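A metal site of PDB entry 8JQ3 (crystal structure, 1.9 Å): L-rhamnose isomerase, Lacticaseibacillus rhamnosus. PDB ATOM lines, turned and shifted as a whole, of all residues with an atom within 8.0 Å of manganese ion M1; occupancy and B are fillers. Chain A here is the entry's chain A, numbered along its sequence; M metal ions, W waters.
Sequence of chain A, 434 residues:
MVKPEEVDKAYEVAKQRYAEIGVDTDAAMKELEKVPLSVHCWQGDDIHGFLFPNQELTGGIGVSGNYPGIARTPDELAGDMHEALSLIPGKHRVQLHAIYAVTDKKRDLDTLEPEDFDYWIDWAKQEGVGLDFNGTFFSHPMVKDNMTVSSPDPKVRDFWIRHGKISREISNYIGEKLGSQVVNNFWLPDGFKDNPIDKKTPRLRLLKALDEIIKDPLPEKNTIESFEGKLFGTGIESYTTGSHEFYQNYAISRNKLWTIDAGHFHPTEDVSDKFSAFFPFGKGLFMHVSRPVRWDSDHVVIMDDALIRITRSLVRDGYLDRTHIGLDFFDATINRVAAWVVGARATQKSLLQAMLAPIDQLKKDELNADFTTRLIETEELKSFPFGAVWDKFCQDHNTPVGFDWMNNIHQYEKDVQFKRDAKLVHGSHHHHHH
Manganese ion M1 is bound by the side-chain carboxylate (OD1) of Asp 296, water W3, water W2, the side-chain carboxylate (OD1) of Asp 298, a ring nitrogen (NE2) of His 264 and water W1. Manganese ion M1 has six donor atoms within binding distance.
The side-chain amino group (NZ) of Lys 230 lies within salt-bridge range of the side-chain carboxylate (OD2) of Asp 296 (3.0 Å). The backbone carbonyl oxygen of Asp 298 sits at hydrogen-bond distance from the backbone NH of Phe 330, 2.9 Å away. The side-chain carboxylate (OE2) of Glu 228 sits close to a ring nitrogen (ND1) of His 264 (3.5 Å).
Water W1 lies within hydrogen-bond range of OD1 of Asp 261 and OG of Ser 290. Water W2 lies within hydrogen-bond range of OD2 of Asp 296 (2.4 Å) and OD2 of Asp 298 (2.7 Å).
Along chain A the residues within 4 Å of manganese ion M1 span positions 264 to 298.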
ATOM      1  N   TRP A 187       4.083  14.968 -41.353  1.00  0.00           N
ATOM      2  CA  TRP A 187       3.588  15.395 -40.018  1.00  0.00           C
ATOM      3  C   TRP A 187       2.918  16.768 -40.150  1.00  0.00           C
ATOM      4  O   TRP A 187       3.540  17.676 -40.732  1.00  0.00           O
ATOM      5  CB  TRP A 187       4.696  15.421 -38.950  1.00  0.00           C
ATOM      6  CG  TRP A 187       4.122  15.935 -37.666  1.00  0.00           C
ATOM      7  CD1 TRP A 187       3.313  15.257 -36.806  1.00  0.00           C
ATOM      8  CD2 TRP A 187       4.220  17.272 -37.148  1.00  0.00           C
ATOM      9  NE1 TRP A 187       2.927  16.067 -35.771  1.00  0.00           N
ATOM     10  CE2 TRP A 187       3.475  17.315 -35.956  1.00  0.00           C
ATOM     11  CE3 TRP A 187       4.881  18.433 -37.577  1.00  0.00           C
ATOM     12  CZ2 TRP A 187       3.374  18.463 -35.180  1.00  0.00           C
ATOM     13  CZ3 TRP A 187       4.770  19.572 -36.804  1.00  0.00           C
ATOM     14  CH2 TRP A 187       4.028  19.581 -35.627  1.00  0.00           C
ATOM     15  N   GLU A 228       2.522  10.515 -39.945  1.00  0.00           N
ATOM     16  CA  GLU A 228       2.960  10.604 -38.527  1.00  0.00           C
ATOM     17  C   GLU A 228       1.866  11.278 -37.683  1.00  0.00           C
ATOM     18  O   GLU A 228       1.603  12.495 -37.875  1.00  0.00           O
ATOM     19  CB  GLU A 228       4.268  11.364 -38.411  1.00  0.00           C
ATOM     20  CG  GLU A 228       4.732  11.523 -36.982  1.00  0.00           C
ATOM     21  CD  GLU A 228       6.087  12.174 -36.836  1.00  0.00           C
ATOM     22  OE1 GLU A 228       6.699  12.503 -37.871  1.00  0.00           O
ATOM     23  OE2 GLU A 228       6.533  12.342 -35.698  1.00  0.00           O
ATOM     24  N   GLY A 229       1.278  10.497 -36.776  1.00  0.00           N
ATOM     25  CA  GLY A 229       0.279  10.970 -35.818  1.00  0.00           C
ATOM     26  C   GLY A 229       0.955  11.552 -34.582  1.00  0.00           C
ATOM     27  O   GLY A 229       2.183  11.390 -34.438  1.00  0.00           O
ATOM     28  N   LYS A 230       0.170  12.231 -33.752  1.00  0.00           N
ATOM     29  CA  LYS A 230       0.573  12.843 -32.461  1.00  0.00           C
ATOM     30  C   LYS A 230      -0.664  12.838 -31.565  1.00  0.00           C
ATOM     31  O   LYS A 230      -1.775  12.930 -32.117  1.00  0.00           O
ATOM     32  CB  LYS A 230       1.098  14.254 -32.719  1.00  0.00           C
ATOM     33  CG  LYS A 230       2.043  14.812 -31.669  1.00  0.00           C
ATOM     34  CD  LYS A 230       2.623  16.140 -32.102  1.00  0.00           C
ATOM     35  CE  LYS A 230       3.629  16.696 -31.135  1.00  0.00           C
ATOM     36  NZ  LYS A 230       4.221  17.945 -31.659  1.00  0.00           N
ATOM     37  N   PHE A 232      -0.828  15.047 -28.701  1.00  0.00           N
ATOM     38  CA  PHE A 232      -0.954  16.469 -28.292  1.00  0.00           C
ATOM     39  C   PHE A 232       0.384  17.199 -28.473  1.00  0.00           C
ATOM     40  O   PHE A 232       1.465  16.594 -28.324  1.00  0.00           O
ATOM     41  CB  PHE A 232      -1.452  16.551 -26.850  1.00  0.00           C
ATOM     42  CG  PHE A 232      -0.386  16.341 -25.806  1.00  0.00           C
ATOM     43  CD1 PHE A 232      -0.016  15.061 -25.429  1.00  0.00           C
ATOM     44  CD2 PHE A 232       0.230  17.420 -25.201  1.00  0.00           C
ATOM     45  CE1 PHE A 232       0.960  14.858 -24.478  1.00  0.00           C
ATOM     46  CE2 PHE A 232       1.205  17.214 -24.236  1.00  0.00           C
ATOM     47  CZ  PHE A 232       1.570  15.932 -23.868  1.00  0.00           C
ATOM     48  N   ASP A 261       6.190   7.704 -33.679  1.00  0.00           N
ATOM     49  CA  ASP A 261       7.178   8.513 -32.922  1.00  0.00           C
ATOM     50  C   ASP A 261       7.004   8.190 -31.439  1.00  0.00           C
ATOM     51  O   ASP A 261       5.905   8.394 -30.904  1.00  0.00           O
ATOM     52  CB  ASP A 261       7.074   9.997 -33.241  1.00  0.00           C
ATOM     53  CG  ASP A 261       8.085  10.854 -32.500  1.00  0.00           C
ATOM     54  OD1 ASP A 261       8.160  10.732 -31.260  1.00  0.00           O
ATOM     55  OD2 ASP A 261       8.819  11.619 -33.164  1.00  0.00           O
ATOM     56  N   ALA A 262       8.057   7.687 -30.801  1.00  0.00           N
ATOM     57  CA  ALA A 262       8.030   7.125 -29.427  1.00  0.00           C
ATOM     58  C   ALA A 262       7.692   8.207 -28.396  1.00  0.00           C
ATOM     59  O   ALA A 262       7.368   7.846 -27.256  1.00  0.00           O
ATOM     60  CB  ALA A 262       9.351   6.457 -29.148  1.00  0.00           C
ATOM     61  N   GLY A 263       7.708   9.476 -28.791  1.00  0.00           N
ATOM     62  CA  GLY A 263       7.440  10.627 -27.905  1.00  0.00           C
ATOM     63  C   GLY A 263       5.994  11.103 -27.957  1.00  0.00           C
ATOM     64  O   GLY A 263       5.634  11.958 -27.142  1.00  0.00           O
ATOM     65  N   HIS A 264       5.180  10.577 -28.877  1.00  0.00           N
ATOM     66  CA  HIS A 264       3.897  11.206 -29.287  1.00  0.00           C
ATOM     67  C   HIS A 264       2.679  10.424 -28.765  1.00  0.00           C
ATOM     68  O   HIS A 264       1.570  10.678 -29.270  1.00  0.00           O
ATOM     69  CB  HIS A 264       3.889  11.390 -30.812  1.00  0.00           C
ATOM     70  CG  HIS A 264       4.903  12.387 -31.279  1.00  0.00           C
ATOM     71  ND1 HIS A 264       5.012  12.774 -32.600  1.00  0.00           N
ATOM     72  CD2 HIS A 264       5.851  13.075 -30.606  1.00  0.00           C
ATOM     73  CE1 HIS A 264       5.984  13.653 -32.719  1.00  0.00           C
ATOM     74  NE2 HIS A 264       6.513  13.861 -31.498  1.00  0.00           N
ATOM     75  N   HIS A 288      10.248   6.332 -35.367  1.00  0.00           N
ATOM     76  CA  HIS A 288      10.971   7.547 -34.902  1.00  0.00           C
ATOM     77  C   HIS A 288      11.266   7.391 -33.410  1.00  0.00           C
ATOM     78  O   HIS A 288      10.343   7.600 -32.596  1.00  0.00           O
ATOM     79  CB  HIS A 288      10.143   8.811 -35.148  1.00  0.00           C
ATOM     80  CG  HIS A 288      10.153   9.288 -36.558  1.00  0.00           C
ATOM     81  ND1 HIS A 288       9.717  10.562 -36.906  1.00  0.00           N
ATOM     82  CD2 HIS A 288      10.571   8.704 -37.705  1.00  0.00           C
ATOM     83  CE1 HIS A 288       9.845  10.716 -38.215  1.00  0.00           C
ATOM     84  NE2 HIS A 288      10.365   9.601 -38.720  1.00  0.00           N
ATOM     85  N   VAL A 289      12.499   7.031 -33.065  1.00  0.00           N
ATOM     86  CA  VAL A 289      12.961   6.971 -31.652  1.00  0.00           C
ATOM     87  C   VAL A 289      13.194   8.399 -31.180  1.00  0.00           C
ATOM     88  O   VAL A 289      13.867   9.188 -31.887  1.00  0.00           O
ATOM     89  CB  VAL A 289      14.184   6.060 -31.469  1.00  0.00           C
ATOM     90  CG1 VAL A 289      13.801   4.593 -31.576  1.00  0.00           C
ATOM     91  CG2 VAL A 289      15.316   6.407 -32.430  1.00  0.00           C
ATOM     92  N   SER A 290      12.617   8.712 -30.025  1.00  0.00           N
ATOM     93  CA  SER A 290      12.599  10.054 -29.392  1.00  0.00           C
ATOM     94  C   SER A 290      12.276   9.831 -27.912  1.00  0.00           C
ATOM     95  O   SER A 290      11.497   8.924 -27.622  1.00  0.00           O
ATOM     96  CB  SER A 290      11.580  10.949 -30.049  1.00  0.00           C
ATOM     97  OG  SER A 290      11.703  12.280 -29.603  1.00  0.00           O
ATOM     98  N   ARG A 291      12.885  10.596 -27.004  1.00  0.00           N
ATOM     99  CA  ARG A 291      12.610  10.430 -25.557  1.00  0.00           C
ATOM    100  C   ARG A 291      11.634  11.513 -25.122  1.00  0.00           C
ATOM    101  O   ARG A 291      11.957  12.704 -25.122  1.00  0.00           O
ATOM    102  CB  ARG A 291      13.916  10.476 -24.743  1.00  0.00           C
ATOM    103  CG  ARG A 291      13.696  10.423 -23.243  1.00  0.00           C
ATOM    104  CD  ARG A 291      14.957  10.066 -22.472  1.00  0.00           C
ATOM    105  NE  ARG A 291      16.093  10.847 -22.921  1.00  0.00           N
ATOM    106  CZ  ARG A 291      16.795  11.699 -22.165  1.00  0.00           C
ATOM    107  NH1 ARG A 291      17.815  12.361 -22.690  1.00  0.00           N
ATOM    108  NH2 ARG A 291      16.484  11.884 -20.901  1.00  0.00           N
ATOM    109  N   PRO A 292      10.397  11.140 -24.738  1.00  0.00           N
ATOM    110  CA  PRO A 292       9.492  12.076 -24.084  1.00  0.00           C
ATOM    111  C   PRO A 292       9.791  12.102 -22.577  1.00  0.00           C
ATOM    112  O   PRO A 292       9.865  11.057 -22.003  1.00  0.00           O
ATOM    113  CB  PRO A 292       8.115  11.459 -24.311  1.00  0.00           C
ATOM    114  CG  PRO A 292       8.391   9.964 -24.330  1.00  0.00           C
ATOM    115  CD  PRO A 292       9.784   9.811 -24.921  1.00  0.00           C
ATOM    116  N   TRP A 295       6.163  14.976 -21.454  1.00  0.00           N
ATOM    117  CA  TRP A 295       5.424  15.486 -22.638  1.00  0.00           C
ATOM    118  C   TRP A 295       6.281  15.231 -23.878  1.00  0.00           C
ATOM    119  O   TRP A 295       7.340  14.596 -23.731  1.00  0.00           O
ATOM    120  CB  TRP A 295       5.053  16.972 -22.477  1.00  0.00           C
ATOM    121  CG  TRP A 295       6.203  17.917 -22.600  1.00  0.00           C
ATOM    122  CD1 TRP A 295       7.244  18.063 -21.721  1.00  0.00           C
ATOM    123  CD2 TRP A 295       6.433  18.874 -23.650  1.00  0.00           C
ATOM    124  NE1 TRP A 295       8.105  19.036 -22.163  1.00  0.00           N
ATOM    125  CE2 TRP A 295       7.632  19.552 -23.337  1.00  0.00           C
ATOM    126  CE3 TRP A 295       5.764  19.218 -24.824  1.00  0.00           C
ATOM    127  CZ2 TRP A 295       8.165  20.546 -24.168  1.00  0.00           C
ATOM    128  CZ3 TRP A 295       6.278  20.195 -25.639  1.00  0.00           C
ATOM    129  CH2 TRP A 295       7.471  20.854 -25.317  1.00  0.00           C
ATOM    130  N   ASP A 296       5.833  15.688 -25.049  1.00  0.00           N
ATOM    131  CA  ASP A 296       6.617  15.559 -26.309  1.00  0.00           C
ATOM    132  C   ASP A 296       7.783  16.551 -26.253  1.00  0.00           C
ATOM    133  O   ASP A 296       7.730  17.580 -26.931  1.00  0.00           O
ATOM    134  CB  ASP A 296       5.714  15.735 -27.523  1.00  0.00           C
ATOM    135  CG  ASP A 296       6.474  15.738 -28.834  1.00  0.00           C
ATOM    136  OD1 ASP A 296       7.506  15.028 -28.911  1.00  0.00           O
ATOM    137  OD2 ASP A 296       6.023  16.451 -29.769  1.00  0.00           O
ATOM    138  N   SER A 297       8.815  16.227 -25.465  1.00  0.00           N
ATOM    139  CA  SER A 297       9.944  17.128 -25.119  1.00  0.00           C
ATOM    140  C   SER A 297      11.118  16.911 -26.066  1.00  0.00           C
ATOM    141  O   SER A 297      12.056  17.727 -26.050  1.00  0.00           O
ATOM    142  CB  SER A 297      10.351  16.918 -23.688  1.00  0.00           C
ATOM    143  OG  SER A 297      10.757  15.580 -23.483  1.00  0.00           O
ATOM    144  N   ASP A 298      11.085  15.842 -26.872  1.00  0.00           N
ATOM    145  CA  ASP A 298      12.093  15.575 -27.934  1.00  0.00           C
ATOM    146  C   ASP A 298      13.503  15.532 -27.322  1.00  0.00           C
ATOM    147  O   ASP A 298      14.436  16.087 -27.931  1.00  0.00           O
ATOM    148  CB  ASP A 298      11.981  16.640 -29.032  1.00  0.00           C
ATOM    149  CG  ASP A 298      10.673  16.560 -29.810  1.00  0.00           C
ATOM    150  OD1 ASP A 298      10.125  15.449 -29.905  1.00  0.00           O
ATOM    151  OD2 ASP A 298      10.198  17.614 -30.271  1.00  0.00           O
ATOM    152  N   HIS A 299      13.657  14.892 -26.162  1.00  0.00           N
ATOM    153  CA  HIS A 299      14.974  14.641 -25.528  1.00  0.00           C
ATOM    154  C   HIS A 299      15.773  13.670 -26.397  1.00  0.00           C
ATOM    155  O   HIS A 299      15.147  12.846 -27.110  1.00  0.00           O
ATOM    156  CB  HIS A 299      14.837  14.099 -24.108  1.00  0.00           C
ATOM    157  CG  HIS A 299      14.565  15.144 -23.080  1.00  0.00           C
ATOM    158  ND1 HIS A 299      13.368  15.830 -23.030  1.00  0.00           N
ATOM    159  CD2 HIS A 299      15.312  15.612 -22.055  1.00  0.00           C
ATOM    160  CE1 HIS A 299      13.384  16.671 -22.024  1.00  0.00           C
ATOM    161  NE2 HIS A 299      14.570  16.563 -21.405  1.00  0.00           N
ATOM    162  N   ASP A 328      14.514  11.275 -34.052  1.00  0.00           N
ATOM    163  CA  ASP A 328      13.727  12.537 -34.010  1.00  0.00           C
ATOM    164  C   ASP A 328      13.794  13.117 -32.596  1.00  0.00           C
ATOM    165  O   ASP A 328      13.055  12.657 -31.699  1.00  0.00           O
ATOM    166  CB  ASP A 328      12.282  12.348 -34.483  1.00  0.00           C
ATOM    167  CG  ASP A 328      11.591  13.671 -34.732  1.00  0.00           C
ATOM    168  OD1 ASP A 328      12.102  14.710 -34.233  1.00  0.00           O
ATOM    169  OD2 ASP A 328      10.543  13.667 -35.410  1.00  0.00           O
ATOM    170  N   PHE A 329      14.652  14.100 -32.415  1.00  0.00           N
ATOM    171  CA  PHE A 329      14.819  14.793 -31.118  1.00  0.00           C
ATOM    172  C   PHE A 329      15.512  16.123 -31.402  1.00  0.00           C
ATOM    173  O   PHE A 329      16.042  16.320 -32.504  1.00  0.00           O
ATOM    174  CB  PHE A 329      15.565  13.905 -30.111  1.00  0.00           C
ATOM    175  CG  PHE A 329      16.889  13.336 -30.559  1.00  0.00           C
ATOM    176  CD1 PHE A 329      18.005  14.139 -30.691  1.00  0.00           C
ATOM    177  CD2 PHE A 329      17.016  11.981 -30.821  1.00  0.00           C
ATOM    178  CE1 PHE A 329      19.224  13.607 -31.089  1.00  0.00           C
ATOM    179  CE2 PHE A 329      18.236  11.450 -31.219  1.00  0.00           C
ATOM    180  CZ  PHE A 329      19.339  12.268 -31.348  1.00  0.00           C
ATOM    181  N   PHE A 330      15.437  17.026 -30.434  1.00  0.00           N
ATOM    182  CA  PHE A 330      15.984  18.391 -30.547  1.00  0.00           C
ATOM    183  C   PHE A 330      16.406  18.830 -29.142  1.00  0.00           C
ATOM    184  O   PHE A 330      15.536  19.159 -28.324  1.00  0.00           O
ATOM    185  CB  PHE A 330      14.964  19.324 -31.203  1.00  0.00           C
ATOM    186  CG  PHE A 330      15.405  20.766 -31.206  1.00  0.00           C
ATOM    187  CD1 PHE A 330      16.731  21.087 -31.470  1.00  0.00           C
ATOM    188  CD2 PHE A 330      14.515  21.786 -30.910  1.00  0.00           C
ATOM    189  CE1 PHE A 330      17.156  22.406 -31.438  1.00  0.00           C
ATOM    190  CE2 PHE A 330      14.947  23.101 -30.892  1.00  0.00           C
ATOM    191  CZ  PHE A 330      16.261  23.411 -31.146  1.00  0.00           C
HETATM  192 MN    MN M   1       8.307  14.755 -30.701  1.00  0.00          MN
HETATM  193 MN    MN M   2       8.716  12.057 -35.418  1.00  0.00          MN
HETATM  194  O   HOH W   1       9.139  12.797 -30.234  1.00  0.00           O
HETATM  195  O   HOH W   2       7.874  16.644 -31.309  1.00  0.00           O
HETATM  196  O   HOH W   3       9.438  14.164 -32.252  1.00  0.00           O
